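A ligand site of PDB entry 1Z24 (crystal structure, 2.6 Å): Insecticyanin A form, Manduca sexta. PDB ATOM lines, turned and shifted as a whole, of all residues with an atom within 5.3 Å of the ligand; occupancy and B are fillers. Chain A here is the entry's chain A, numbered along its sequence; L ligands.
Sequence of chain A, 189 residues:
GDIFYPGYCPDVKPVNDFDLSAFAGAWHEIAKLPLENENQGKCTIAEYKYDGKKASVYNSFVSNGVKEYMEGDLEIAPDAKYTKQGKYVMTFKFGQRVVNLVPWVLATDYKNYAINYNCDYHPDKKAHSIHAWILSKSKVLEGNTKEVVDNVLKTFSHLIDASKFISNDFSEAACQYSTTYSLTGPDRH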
ATOM      1  N   GLU A  29     -35.935 -30.195  21.562  1.00  0.00           N
ATOM      2  CA  GLU A  29     -35.738 -29.392  22.765  1.00  0.00           C
ATOM      3  C   GLU A  29     -37.043 -28.669  23.069  1.00  0.00           C
ATOM      4  O   GLU A  29     -37.293 -27.645  22.511  1.00  0.00           O
ATOM      5  CB  GLU A  29     -34.602 -28.413  22.497  1.00  0.00           C
ATOM      6  CG  GLU A  29     -34.518 -27.385  23.642  1.00  0.00           C
ATOM      7  CD  GLU A  29     -33.441 -26.430  23.342  1.00  0.00           C
ATOM      8  OE1 GLU A  29     -32.254 -26.706  23.501  1.00  0.00           O
ATOM      9  OE2 GLU A  29     -33.904 -25.327  22.849  1.00  0.00           O
ATOM     10  N   LEU A  35     -29.327 -20.232  27.328  1.00  0.00           N
ATOM     11  CA  LEU A  35     -27.982 -20.674  26.925  1.00  0.00           C
ATOM     12  C   LEU A  35     -27.560 -19.820  25.733  1.00  0.00           C
ATOM     13  O   LEU A  35     -28.169 -19.952  24.665  1.00  0.00           O
ATOM     14  CB  LEU A  35     -27.923 -22.191  26.674  1.00  0.00           C
ATOM     15  CG  LEU A  35     -26.570 -22.694  26.110  1.00  0.00           C
ATOM     16  CD1 LEU A  35     -25.394 -22.245  27.017  1.00  0.00           C
ATOM     17  CD2 LEU A  35     -26.593 -24.219  25.944  1.00  0.00           C
ATOM     18  N   ASN A  37     -25.327 -19.578  23.335  1.00  0.00           N
ATOM     19  CA  ASN A  37     -25.137 -20.081  22.009  1.00  0.00           C
ATOM     20  C   ASN A  37     -26.367 -20.534  21.367  1.00  0.00           C
ATOM     21  O   ASN A  37     -26.345 -20.706  20.176  1.00  0.00           O
ATOM     22  CB  ASN A  37     -24.034 -21.145  21.841  1.00  0.00           C
ATOM     23  CG  ASN A  37     -24.374 -22.439  22.589  1.00  0.00           C
ATOM     24  OD1 ASN A  37     -25.522 -22.898  22.611  1.00  0.00           O
ATOM     25  ND2 ASN A  37     -23.367 -23.129  23.078  1.00  0.00           N
ATOM     26  N   GLU A  38     -27.430 -20.787  22.086  1.00  0.00           N
ATOM     27  CA  GLU A  38     -28.545 -21.274  21.309  1.00  0.00           C
ATOM     28  C   GLU A  38     -29.876 -20.554  21.517  1.00  0.00           C
ATOM     29  O   GLU A  38     -30.971 -20.977  21.080  1.00  0.00           O
ATOM     30  CB  GLU A  38     -28.605 -22.756  21.511  1.00  0.00           C
ATOM     31  CG  GLU A  38     -29.078 -23.087  22.982  1.00  0.00           C
ATOM     32  CD  GLU A  38     -29.449 -24.560  23.093  1.00  0.00           C
ATOM     33  OE1 GLU A  38     -28.861 -25.420  23.680  1.00  0.00           O
ATOM     34  OE2 GLU A  38     -30.549 -24.823  22.489  1.00  0.00           O
ATOM     35  N   THR A  44     -35.189 -26.535  17.494  1.00  0.00           N
ATOM     36  CA  THR A  44     -33.949 -27.180  17.923  1.00  0.00           C
ATOM     37  C   THR A  44     -34.055 -28.676  18.190  1.00  0.00           C
ATOM     38  O   THR A  44     -34.829 -29.114  19.032  1.00  0.00           O
ATOM     39  CB  THR A  44     -33.496 -26.514  19.208  1.00  0.00           C
ATOM     40  OG1 THR A  44     -33.472 -25.204  18.899  1.00  0.00           O
ATOM     41  CG2 THR A  44     -32.062 -26.951  19.578  1.00  0.00           C
ATOM     42  N   ILE A  45     -33.246 -29.457  17.483  1.00  0.00           N
ATOM     43  CA  ILE A  45     -33.279 -30.884  17.661  1.00  0.00           C
ATOM     44  C   ILE A  45     -31.873 -31.468  17.670  1.00  0.00           C
ATOM     45  O   ILE A  45     -30.997 -31.114  16.880  1.00  0.00           O
ATOM     46  CB  ILE A  45     -33.988 -31.430  16.444  1.00  0.00           C
ATOM     47  CG1 ILE A  45     -35.306 -30.706  16.232  1.00  0.00           C
ATOM     48  CG2 ILE A  45     -34.100 -32.968  16.507  1.00  0.00           C
ATOM     49  CD1 ILE A  45     -36.042 -31.212  15.011  1.00  0.00           C
ATOM     50  N   ALA A  46     -31.639 -32.372  18.574  1.00  0.00           N
ATOM     51  CA  ALA A  46     -30.351 -33.024  18.671  1.00  0.00           C
ATOM     52  C   ALA A  46     -30.572 -34.466  18.274  1.00  0.00           C
ATOM     53  O   ALA A  46     -31.417 -35.143  18.882  1.00  0.00           O
ATOM     54  CB  ALA A  46     -29.793 -32.972  20.104  1.00  0.00           C
ATOM     55  N   TYR A  48     -28.893 -38.222  17.879  1.00  0.00           N
ATOM     56  CA  TYR A  48     -27.819 -39.079  18.237  1.00  0.00           C
ATOM     57  C   TYR A  48     -28.045 -40.395  17.561  1.00  0.00           C
ATOM     58  O   TYR A  48     -29.140 -40.911  17.652  1.00  0.00           O
ATOM     59  CB  TYR A  48     -27.823 -39.351  19.784  1.00  0.00           C
ATOM     60  CG  TYR A  48     -27.775 -38.050  20.639  1.00  0.00           C
ATOM     61  CD1 TYR A  48     -26.989 -36.963  20.238  1.00  0.00           C
ATOM     62  CD2 TYR A  48     -28.568 -37.866  21.776  1.00  0.00           C
ATOM     63  CE1 TYR A  48     -26.930 -35.782  20.965  1.00  0.00           C
ATOM     64  CE2 TYR A  48     -28.514 -36.694  22.535  1.00  0.00           C
ATOM     65  CZ  TYR A  48     -27.684 -35.648  22.130  1.00  0.00           C
ATOM     66  OH  TYR A  48     -27.564 -34.470  22.852  1.00  0.00           O
ATOM     67  N   ASN A  59     -26.606 -31.902  15.339  1.00  0.00           N
ATOM     68  CA  ASN A  59     -27.442 -30.917  15.990  1.00  0.00           C
ATOM     69  C   ASN A  59     -27.858 -29.834  15.001  1.00  0.00           C
ATOM     70  O   ASN A  59     -27.061 -29.366  14.152  1.00  0.00           O
ATOM     71  CB  ASN A  59     -26.631 -30.122  17.048  1.00  0.00           C
ATOM     72  CG  ASN A  59     -26.400 -30.732  18.425  1.00  0.00           C
ATOM     73  OD1 ASN A  59     -27.154 -31.639  18.898  1.00  0.00           O
ATOM     74  ND2 ASN A  59     -25.275 -30.205  19.088  1.00  0.00           N
ATOM     75  N   SER A  60     -29.089 -29.394  15.118  1.00  0.00           N
ATOM     76  CA  SER A  60     -29.553 -28.366  14.255  1.00  0.00           C
ATOM     77  C   SER A  60     -30.660 -27.533  14.817  1.00  0.00           C
ATOM     78  O   SER A  60     -31.415 -27.915  15.688  1.00  0.00           O
ATOM     79  CB  SER A  60     -30.015 -28.902  12.885  1.00  0.00           C
ATOM     80  OG  SER A  60     -31.336 -29.479  12.943  1.00  0.00           O
ATOM     81  N   PHE A  61     -30.741 -26.369  14.242  1.00  0.00           N
ATOM     82  CA  PHE A  61     -31.748 -25.402  14.559  1.00  0.00           C
ATOM     83  C   PHE A  61     -31.880 -24.460  13.398  1.00  0.00           C
ATOM     84  O   PHE A  61     -31.077 -24.467  12.459  1.00  0.00           O
ATOM     85  CB  PHE A  61     -31.692 -24.765  15.921  1.00  0.00           C
ATOM     86  CG  PHE A  61     -30.461 -23.961  16.244  1.00  0.00           C
ATOM     87  CD1 PHE A  61     -29.718 -23.260  15.271  1.00  0.00           C
ATOM     88  CD2 PHE A  61     -30.068 -23.860  17.584  1.00  0.00           C
ATOM     89  CE1 PHE A  61     -28.611 -22.484  15.617  1.00  0.00           C
ATOM     90  CE2 PHE A  61     -28.969 -23.069  17.939  1.00  0.00           C
ATOM     91  CZ  PHE A  61     -28.224 -22.381  16.969  1.00  0.00           C
ATOM     92  N   GLU A  68     -28.936 -24.055  10.669  1.00  0.00           N
ATOM     93  CA  GLU A  68     -27.569 -24.260  11.088  1.00  0.00           C
ATOM     94  C   GLU A  68     -27.401 -25.587  11.806  1.00  0.00           C
ATOM     95  O   GLU A  68     -28.233 -26.030  12.648  1.00  0.00           O
ATOM     96  CB  GLU A  68     -27.050 -23.120  11.938  1.00  0.00           C
ATOM     97  CG  GLU A  68     -27.184 -21.817  11.186  1.00  0.00           C
ATOM     98  CD  GLU A  68     -26.870 -20.665  12.088  1.00  0.00           C
ATOM     99  OE1 GLU A  68     -26.426 -20.811  13.207  1.00  0.00           O
ATOM    100  OE2 GLU A  68     -27.126 -19.507  11.561  1.00  0.00           O
ATOM    101  N   TYR A  69     -26.283 -26.240  11.460  1.00  0.00           N
ATOM    102  CA  TYR A  69     -26.062 -27.507  12.086  1.00  0.00           C
ATOM    103  C   TYR A  69     -24.617 -27.775  12.468  1.00  0.00           C
ATOM    104  O   TYR A  69     -23.696 -27.059  12.064  1.00  0.00           O
ATOM    105  CB  TYR A  69     -26.644 -28.598  11.211  1.00  0.00           C
ATOM    106  CG  TYR A  69     -25.929 -28.648   9.923  1.00  0.00           C
ATOM    107  CD1 TYR A  69     -24.935 -29.627   9.797  1.00  0.00           C
ATOM    108  CD2 TYR A  69     -26.235 -27.775   8.866  1.00  0.00           C
ATOM    109  CE1 TYR A  69     -24.239 -29.752   8.589  1.00  0.00           C
ATOM    110  CE2 TYR A  69     -25.550 -27.874   7.648  1.00  0.00           C
ATOM    111  CZ  TYR A  69     -24.557 -28.873   7.532  1.00  0.00           C
ATOM    112  OH  TYR A  69     -23.846 -29.032   6.369  1.00  0.00           O
ATOM    113  N   MET A  70     -24.448 -28.828  13.286  1.00  0.00           N
ATOM    114  CA  MET A  70     -23.140 -29.235  13.768  1.00  0.00           C
ATOM    115  C   MET A  70     -23.069 -30.734  13.760  1.00  0.00           C
ATOM    116  O   MET A  70     -24.030 -31.401  14.176  1.00  0.00           O
ATOM    117  CB  MET A  70     -23.046 -28.945  15.274  1.00  0.00           C
ATOM    118  CG  MET A  70     -23.181 -27.508  15.646  1.00  0.00           C
ATOM    119  SD  MET A  70     -23.505 -27.260  17.417  1.00  0.00           S
ATOM    120  CE  MET A  70     -21.925 -27.418  18.184  1.00  0.00           C
ATOM    121  N   TYR A  88     -22.405 -37.996  28.962  1.00  0.00           N
ATOM    122  CA  TYR A  88     -21.762 -38.195  27.683  1.00  0.00           C
ATOM    123  C   TYR A  88     -21.012 -36.970  27.179  1.00  0.00           C
ATOM    124  O   TYR A  88     -21.212 -35.830  27.614  1.00  0.00           O
ATOM    125  CB  TYR A  88     -22.778 -38.813  26.667  1.00  0.00           C
ATOM    126  CG  TYR A  88     -23.931 -37.908  26.331  1.00  0.00           C
ATOM    127  CD1 TYR A  88     -23.878 -37.024  25.251  1.00  0.00           C
ATOM    128  CD2 TYR A  88     -25.067 -37.890  27.158  1.00  0.00           C
ATOM    129  CE1 TYR A  88     -24.954 -36.187  24.902  1.00  0.00           C
ATOM    130  CE2 TYR A  88     -26.137 -37.058  26.863  1.00  0.00           C
ATOM    131  CZ  TYR A  88     -26.076 -36.223  25.743  1.00  0.00           C
ATOM    132  OH  TYR A  88     -27.149 -35.397  25.496  1.00  0.00           O
ATOM    133  N   MET A  90     -19.737 -34.799  23.710  1.00  0.00           N
ATOM    134  CA  MET A  90     -19.964 -34.455  22.325  1.00  0.00           C
ATOM    135  C   MET A  90     -18.753 -33.644  21.914  1.00  0.00           C
ATOM    136  O   MET A  90     -18.440 -32.650  22.555  1.00  0.00           O
ATOM    137  CB  MET A  90     -21.210 -33.634  22.184  1.00  0.00           C
ATOM    138  CG  MET A  90     -22.413 -34.478  22.612  1.00  0.00           C
ATOM    139  SD  MET A  90     -23.937 -33.575  22.194  1.00  0.00           S
ATOM    140  CE  MET A  90     -23.898 -32.120  23.329  1.00  0.00           C
ATOM    141  N   PHE A  94     -14.031 -26.899  15.184  1.00  0.00           N
ATOM    142  CA  PHE A  94     -14.231 -25.717  14.382  1.00  0.00           C
ATOM    143  C   PHE A  94     -12.828 -25.451  13.964  1.00  0.00           C
ATOM    144  O   PHE A  94     -12.079 -24.876  14.766  1.00  0.00           O
ATOM    145  CB  PHE A  94     -14.699 -24.622  15.291  1.00  0.00           C
ATOM    146  CG  PHE A  94     -15.958 -25.084  15.889  1.00  0.00           C
ATOM    147  CD1 PHE A  94     -15.889 -25.733  17.111  1.00  0.00           C
ATOM    148  CD2 PHE A  94     -17.176 -24.892  15.229  1.00  0.00           C
ATOM    149  CE1 PHE A  94     -17.060 -26.190  17.735  1.00  0.00           C
ATOM    150  CE2 PHE A  94     -18.353 -25.344  15.840  1.00  0.00           C
ATOM    151  CZ  PHE A  94     -18.273 -25.989  17.084  1.00  0.00           C
ATOM    152  N   ARG A  97     -10.113 -25.481  16.603  1.00  0.00           N
ATOM    153  CA  ARG A  97     -10.727 -25.449  17.902  1.00  0.00           C
ATOM    154  C   ARG A  97     -11.535 -26.706  18.105  1.00  0.00           C
ATOM    155  O   ARG A  97     -12.383 -27.080  17.272  1.00  0.00           O
ATOM    156  CB  ARG A  97     -11.590 -24.199  18.080  1.00  0.00           C
ATOM    157  CG  ARG A  97     -12.265 -24.213  19.440  1.00  0.00           C
ATOM    158  CD  ARG A  97     -12.821 -22.831  19.691  1.00  0.00           C
ATOM    159  NE  ARG A  97     -13.720 -22.506  18.584  1.00  0.00           N
ATOM    160  CZ  ARG A  97     -15.023 -22.571  18.676  1.00  0.00           C
ATOM    161  NH1 ARG A  97     -15.606 -22.944  19.818  1.00  0.00           N
ATOM    162  NH2 ARG A  97     -15.785 -22.255  17.617  1.00  0.00           N
ATOM    163  N   VAL A  99     -14.043 -28.698  20.759  1.00  0.00           N
ATOM    164  CA  VAL A  99     -14.950 -28.554  21.884  1.00  0.00           C
ATOM    165  C   VAL A  99     -15.451 -29.931  22.385  1.00  0.00           C
ATOM    166  O   VAL A  99     -15.808 -30.816  21.600  1.00  0.00           O
ATOM    167  CB  VAL A  99     -16.054 -27.655  21.357  1.00  0.00           C
ATOM    168  CG1 VAL A  99     -17.231 -27.725  22.285  1.00  0.00           C
ATOM    169  CG2 VAL A  99     -15.522 -26.206  21.194  1.00  0.00           C
ATOM    170  N   LEU A 101     -18.308 -31.093  24.840  1.00  0.00           N
ATOM    171  CA  LEU A 101     -19.490 -30.795  25.642  1.00  0.00           C
ATOM    172  C   LEU A 101     -19.938 -32.005  26.432  1.00  0.00           C
ATOM    173  O   LEU A 101     -19.958 -33.159  25.938  1.00  0.00           O
ATOM    174  CB  LEU A 101     -20.666 -30.188  24.859  1.00  0.00           C
ATOM    175  CG  LEU A 101     -20.219 -29.028  23.942  1.00  0.00           C
ATOM    176  CD1 LEU A 101     -21.419 -28.518  23.149  1.00  0.00           C
ATOM    177  CD2 LEU A 101     -19.679 -27.863  24.809  1.00  0.00           C
ATOM    178  N   VAL A 102     -20.336 -31.719  27.680  1.00  0.00           N
ATOM    179  CA  VAL A 102     -20.736 -32.763  28.537  1.00  0.00           C
ATOM    180  C   VAL A 102     -22.079 -32.634  29.224  1.00  0.00           C
ATOM    181  O   VAL A 102     -22.120 -32.158  30.352  1.00  0.00           O
ATOM    182  CB  VAL A 102     -19.607 -32.987  29.617  1.00  0.00           C
ATOM    183  CG1 VAL A 102     -19.932 -34.187  30.495  1.00  0.00           C
ATOM    184  CG2 VAL A 102     -18.219 -33.188  29.039  1.00  0.00           C
ATOM    185  N   PRO A 103     -23.144 -33.086  28.595  1.00  0.00           N
ATOM    186  CA  PRO A 103     -24.420 -33.012  29.261  1.00  0.00           C
ATOM    187  C   PRO A 103     -24.607 -34.157  30.269  1.00  0.00           C
ATOM    188  O   PRO A 103     -24.177 -35.281  30.080  1.00  0.00           O
ATOM    189  CB  PRO A 103     -25.459 -33.206  28.174  1.00  0.00           C
ATOM    190  CG  PRO A 103     -24.691 -33.243  26.849  1.00  0.00           C
ATOM    191  CD  PRO A 103     -23.286 -33.660  27.224  1.00  0.00           C
ATOM    192  N   ASN A 116     -31.829 -33.210  30.813  1.00  0.00           N
ATOM    193  CA  ASN A 116     -30.378 -32.999  30.741  1.00  0.00           C
ATOM    194  C   ASN A 116     -29.951 -31.737  31.467  1.00  0.00           C
ATOM    195  O   ASN A 116     -30.734 -30.792  31.578  1.00  0.00           O
ATOM    196  CB  ASN A 116     -29.901 -32.969  29.273  1.00  0.00           C
ATOM    197  CG  ASN A 116     -29.814 -34.353  28.679  1.00  0.00           C
ATOM    198  OD1 ASN A 116     -29.164 -34.579  27.668  1.00  0.00           O
ATOM    199  ND2 ASN A 116     -30.442 -35.263  29.282  1.00  0.00           N
ATOM    200  N   ASN A 118     -26.267 -29.262  33.138  1.00  0.00           N
ATOM    201  CA  ASN A 118     -24.845 -29.002  33.248  1.00  0.00           C
ATOM    202  C   ASN A 118     -24.655 -27.848  34.227  1.00  0.00           C
ATOM    203  O   ASN A 118     -25.595 -27.117  34.478  1.00  0.00           O
ATOM    204  CB  ASN A 118     -23.935 -28.944  32.035  1.00  0.00           C
ATOM    205  CG  ASN A 118     -23.636 -27.531  31.594  1.00  0.00           C
ATOM    206  OD1 ASN A 118     -24.537 -26.722  31.334  1.00  0.00           O
ATOM    207  ND2 ASN A 118     -22.360 -27.258  31.463  1.00  0.00           N
ATOM    208  N   ASP A 120     -21.553 -25.064  35.099  1.00  0.00           N
ATOM    209  CA  ASP A 120     -20.286 -24.479  34.680  1.00  0.00           C
ATOM    210  C   ASP A 120     -19.767 -23.523  35.732  1.00  0.00           C
ATOM    211  O   ASP A 120     -20.376 -22.463  35.972  1.00  0.00           O
ATOM    212  CB  ASP A 120     -20.633 -23.735  33.385  1.00  0.00           C
ATOM    213  CG  ASP A 120     -19.427 -23.251  32.606  1.00  0.00           C
ATOM    214  OD1 ASP A 120     -19.380 -23.288  31.391  1.00  0.00           O
ATOM    215  OD2 ASP A 120     -18.411 -22.837  33.335  1.00  0.00           O
ATOM    216  N   SER A 129     -22.916 -21.132  36.412  1.00  0.00           N
ATOM    217  CA  SER A 129     -24.103 -20.969  35.601  1.00  0.00           C
ATOM    218  C   SER A 129     -24.749 -22.357  35.494  1.00  0.00           C
ATOM    219  O   SER A 129     -24.062 -23.374  35.557  1.00  0.00           O
ATOM    220  CB  SER A 129     -23.914 -20.397  34.208  1.00  0.00           C
ATOM    221  OG  SER A 129     -22.869 -21.065  33.501  1.00  0.00           O
ATOM    222  N   HIS A 131     -27.341 -24.897  33.213  1.00  0.00           N
ATOM    223  CA  HIS A 131     -28.036 -25.088  31.964  1.00  0.00           C
ATOM    224  C   HIS A 131     -28.910 -26.333  32.054  1.00  0.00           C
ATOM    225  O   HIS A 131     -28.523 -27.305  32.684  1.00  0.00           O
ATOM    226  CB  HIS A 131     -27.169 -25.167  30.726  1.00  0.00           C
ATOM    227  CG  HIS A 131     -26.273 -23.992  30.723  1.00  0.00           C
ATOM    228  ND1 HIS A 131     -24.939 -24.067  31.116  1.00  0.00           N
ATOM    229  CD2 HIS A 131     -26.542 -22.701  30.403  1.00  0.00           C
ATOM    230  CE1 HIS A 131     -24.449 -22.787  30.998  1.00  0.00           C
ATOM    231  NE2 HIS A 131     -25.377 -21.950  30.570  1.00  0.00           N
ATOM    232  N   TRP A 133     -32.214 -28.806  29.847  1.00  0.00           N
ATOM    233  CA  TRP A 133     -33.046 -29.006  28.659  1.00  0.00           C
ATOM    234  C   TRP A 133     -34.080 -30.081  28.817  1.00  0.00           C
ATOM    235  O   TRP A 133     -33.799 -31.186  29.303  1.00  0.00           O
ATOM    236  CB  TRP A 133     -32.196 -29.594  27.527  1.00  0.00           C
ATOM    237  CG  TRP A 133     -31.069 -28.761  27.072  1.00  0.00           C
ATOM    238  CD1 TRP A 133     -31.044 -27.983  25.931  1.00  0.00           C
ATOM    239  CD2 TRP A 133     -29.769 -28.637  27.735  1.00  0.00           C
ATOM    240  NE1 TRP A 133     -29.768 -27.369  25.859  1.00  0.00           N
ATOM    241  CE2 TRP A 133     -28.979 -27.729  26.946  1.00  0.00           C
ATOM    242  CE3 TRP A 133     -29.241 -29.180  28.932  1.00  0.00           C
ATOM    243  CZ2 TRP A 133     -27.624 -27.368  27.310  1.00  0.00           C
ATOM    244  CZ3 TRP A 133     -27.962 -28.848  29.337  1.00  0.00           C
ATOM    245  CH2 TRP A 133     -27.152 -27.964  28.521  1.00  0.00           C
ATOM    246  N   LEU A 135     -36.089 -32.610  26.962  1.00  0.00           N
ATOM    247  CA  LEU A 135     -36.076 -33.205  25.651  1.00  0.00           C
ATOM    248  C   LEU A 135     -37.141 -34.270  25.446  1.00  0.00           C
ATOM    249  O   LEU A 135     -37.431 -35.055  26.337  1.00  0.00           O
ATOM    250  CB  LEU A 135     -34.719 -33.951  25.405  1.00  0.00           C
ATOM    251  CG  LEU A 135     -33.517 -33.093  25.721  1.00  0.00           C
ATOM    252  CD1 LEU A 135     -32.331 -34.000  25.542  1.00  0.00           C
ATOM    253  CD2 LEU A 135     -33.473 -32.016  24.679  1.00  0.00           C
ATOM    254  N   LEU A 183     -21.998 -25.273  11.034  1.00  0.00           N
ATOM    255  CA  LEU A 183     -21.203 -24.507  11.963  1.00  0.00           C
ATOM    256  C   LEU A 183     -19.867 -25.161  12.203  1.00  0.00           C
ATOM    257  O   LEU A 183     -18.909 -24.499  12.500  1.00  0.00           O
ATOM    258  CB  LEU A 183     -21.920 -24.366  13.330  1.00  0.00           C
ATOM    259  CG  LEU A 183     -23.254 -23.628  13.205  1.00  0.00           C
ATOM    260  CD1 LEU A 183     -24.008 -23.836  14.435  1.00  0.00           C
ATOM    261  CD2 LEU A 183     -23.029 -22.148  13.083  1.00  0.00           C
ATOM    262  N   HIS A 189     -13.504 -21.550  12.887  1.00  0.00           N
ATOM    263  CA  HIS A 189     -12.632 -21.232  13.986  1.00  0.00           C
ATOM    264  C   HIS A 189     -13.319 -21.175  15.306  1.00  0.00           C
ATOM    265  O   HIS A 189     -12.528 -21.070  16.284  1.00  0.00           O
ATOM    266  CB  HIS A 189     -11.736 -19.987  13.795  1.00  0.00           C
ATOM    267  CG  HIS A 189     -12.486 -18.754  13.547  1.00  0.00           C
ATOM    268  ND1 HIS A 189     -13.029 -18.500  12.302  1.00  0.00           N
ATOM    269  CD2 HIS A 189     -12.770 -17.701  14.370  1.00  0.00           C
ATOM    270  CE1 HIS A 189     -13.634 -17.297  12.364  1.00  0.00           C
ATOM    271  NE2 HIS A 189     -13.491 -16.800  13.612  1.00  0.00           N
ATOM    272  OXT HIS A 189     -14.586 -21.231  15.311  1.00  0.00           O
HETATM  273  N1  LIG L   1     -24.635 -27.100  24.731  1.00  0.00           N
HETATM  274  C1  LIG L   1     -23.678 -26.349  25.312  1.00  0.00           C
HETATM  275  C2  LIG L   1     -23.076 -26.969  26.486  1.00  0.00           C
HETATM  276  C3  LIG L   1     -23.711 -28.174  26.611  1.00  0.00           C
HETATM  277  C4  LIG L   1     -24.686 -28.234  25.513  1.00  0.00           C
HETATM  278  C5  LIG L   1     -23.548 -29.279  27.727  1.00  0.00           C
HETATM  279  O1  LIG L   1     -23.348 -25.263  24.878  1.00  0.00           O
HETATM  280  C6  LIG L   1     -22.057 -26.373  27.359  1.00  0.00           C
HETATM  281  C7  LIG L   1     -22.839 -25.391  28.182  1.00  0.00           C
HETATM  282  C8  LIG L   1     -21.856 -24.542  28.997  1.00  0.00           C
HETATM  283  O2  LIG L   1     -21.674 -24.745  30.167  1.00  0.00           O
HETATM  284  O3  LIG L   1     -21.238 -23.688  28.451  1.00  0.00           O
HETATM  285  C9  LIG L   1     -25.561 -29.313  25.345  1.00  0.00           C
HETATM  286  N2  LIG L   1     -26.780 -28.700  23.306  1.00  0.00           N
HETATM  287  C10 LIG L   1     -26.640 -29.415  24.487  1.00  0.00           C
HETATM  288  C11 LIG L   1     -27.758 -30.306  24.674  1.00  0.00           C
HETATM  289  C12 LIG L   1     -28.551 -30.120  23.628  1.00  0.00           C
HETATM  290  C13 LIG L   1     -27.941 -29.094  22.771  1.00  0.00           C
HETATM  291  C14 LIG L   1     -27.950 -31.267  25.839  1.00  0.00           C
HETATM  292  C15 LIG L   1     -29.857 -30.819  23.364  1.00  0.00           C
HETATM  293  C16 LIG L   1     -30.828 -29.989  22.872  1.00  0.00           C
HETATM  294  C17 LIG L   1     -28.476 -28.678  21.544  1.00  0.00           C
HETATM  295  N3  LIG L   1     -27.060 -26.909  20.690  1.00  0.00           N
HETATM  296  C18 LIG L   1     -28.006 -27.874  20.550  1.00  0.00           C
HETATM  297  C19 LIG L   1     -28.517 -27.926  19.177  1.00  0.00           C
HETATM  298  C20 LIG L   1     -27.884 -27.035  18.406  1.00  0.00           C
HETATM  299  C21 LIG L   1     -26.938 -26.364  19.385  1.00  0.00           C
HETATM  300  C22 LIG L   1     -29.481 -28.905  18.700  1.00  0.00           C
HETATM  301  C23 LIG L   1     -27.990 -26.618  16.927  1.00  0.00           C
HETATM  302  C24 LIG L   1     -26.943 -26.059  16.286  1.00  0.00           C
HETATM  303  C25 LIG L   1     -26.082 -25.249  19.078  1.00  0.00           C
HETATM  304  N4  LIG L   1     -24.170 -25.812  20.543  1.00  0.00           N
HETATM  305  C26 LIG L   1     -24.821 -24.989  19.580  1.00  0.00           C
HETATM  306  C27 LIG L   1     -23.914 -23.864  19.178  1.00  0.00           C
HETATM  307  C28 LIG L   1     -22.747 -24.001  19.893  1.00  0.00           C
HETATM  308  C29 LIG L   1     -22.944 -25.193  20.704  1.00  0.00           C
HETATM  309  C30 LIG L   1     -24.205 -22.753  18.209  1.00  0.00           C
HETATM  310  O4  LIG L   1     -22.089 -25.619  21.444  1.00  0.00           O
HETATM  311  C31 LIG L   1     -21.566 -23.129  19.826  1.00  0.00           C
HETATM  312  C32 LIG L   1     -20.512 -23.838  18.990  1.00  0.00           C
HETATM  313  C33 LIG L   1     -19.134 -23.081  19.043  1.00  0.00           C
HETATM  314  O5  LIG L   1     -18.847 -22.303  18.200  1.00  0.00           O
HETATM  315  O6  LIG L   1     -18.347 -23.261  19.953  1.00  0.00           O
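The side-chain carboxylate (OD1) of Asp 120 lies close to an oxygen (O2) of the ligand (3.0 Å). An oxygen (O2) of the ligand sits at hydrogen-bond distance from a ring nitrogen (ND1) of His 131 (3.5 Å). ND2 of Asn 118 is in hydrogen-bond range of O2 of the ligand (2.9 Å). An oxygen (O1) of the ligand sits at hydrogen-bond distance from the side-chain amide nitrogen of Asn 37, at 2.8 Å. An oxygen (O6) of the ligand is in salt-bridge range of the guanidinium group (NH1) of Arg 97 (2.8 Å).
The chain-end carboxylate of His 189 is in salt-bridge range of the guanidinium group of Arg 97 (2.8 Å). The backbone carbonyl oxygen of Phe 61 lies within hydrogen-bond range of the backbone NH of Glu 68 (2.8 Å). O of Thr 44 sits at hydrogen-bond distance from N of Glu 29 (3.0 Å). OD1 of Asn 118 is in hydrogen-bond range of ND1 of His 131. NE1 of Trp 133 lies close to OE1 of Glu 29 (3.5 Å). The backbone NH of Tyr 88 is in hydrogen-bond range of the backbone carbonyl oxygen of Pro 103 (3.4 Å). OD1 of Asn 116 lies within hydrogen-bond range of OH of Tyr 88 (3.1 Å). The backbone carbonyl oxygen (O) of Asn 116 lies within hydrogen-bond range of the backbone NH (N) of Trp 133, 3.0 Å away.
N4 of the ligand sits close to SD of Met 70, at 3.5 Å. OE1 of Glu 29 touches C16 of the ligand, at 3.6 Å. Leu 35 touches the ligand. Glu 38 touches the ligand (OE1 to N3, 3.8 Å). Thr 44 touches the ligand. O of Ile 45 touches C22 of the ligand, 3.2 Å away. Ala 46 touches the ligand (CB to C15, 3.9 Å). CB of Asn 59 touches C22 of the ligand, at 3.5 Å. N of Ser 60 touches C23 of the ligand, at 3.5 Å. Phe 61 touches the ligand. Glu 68 touches the ligand. Met 90 touches the ligand. Phe 94 touches the ligand (CZ to C33, 3.6 Å). CD1 of Leu 101 touches O4 of the ligand, 3.4 Å away. Val 102 touches the ligand (C to C5, 3.96 Å). Pro 103 touches the ligand. OD1 of Asn 116 touches C14 of the ligand, 3.97 Å away. Trp 133 touches the ligand. Leu 135 touches the ligand. Leu 183 touches the ligand (CD1 to C30, 3.9 Å). Hydrophobic or aromatic side chains within 4 Å of the ligand: Leu 35, Ala 46, Phe 61, Met 70, Met 90, Phe 94, Leu 101, Pro 103, His 131, Trp 133, Leu 135 and Leu 183. 25 residues have an atom within 4 Å of the ligand: Glu 29, Leu 35, Asn 37, Glu 38, Thr 44, Ile 45, Ala 46, Asn 59, Ser 60, Phe 61, Glu 68, Met 70, Met 90, Phe 94, Arg 97, Leu 101, Val 102, Pro 103, Asn 116, Asn 118, Asp 120, His 131, Trp 133, Leu 135 and Leu 183.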
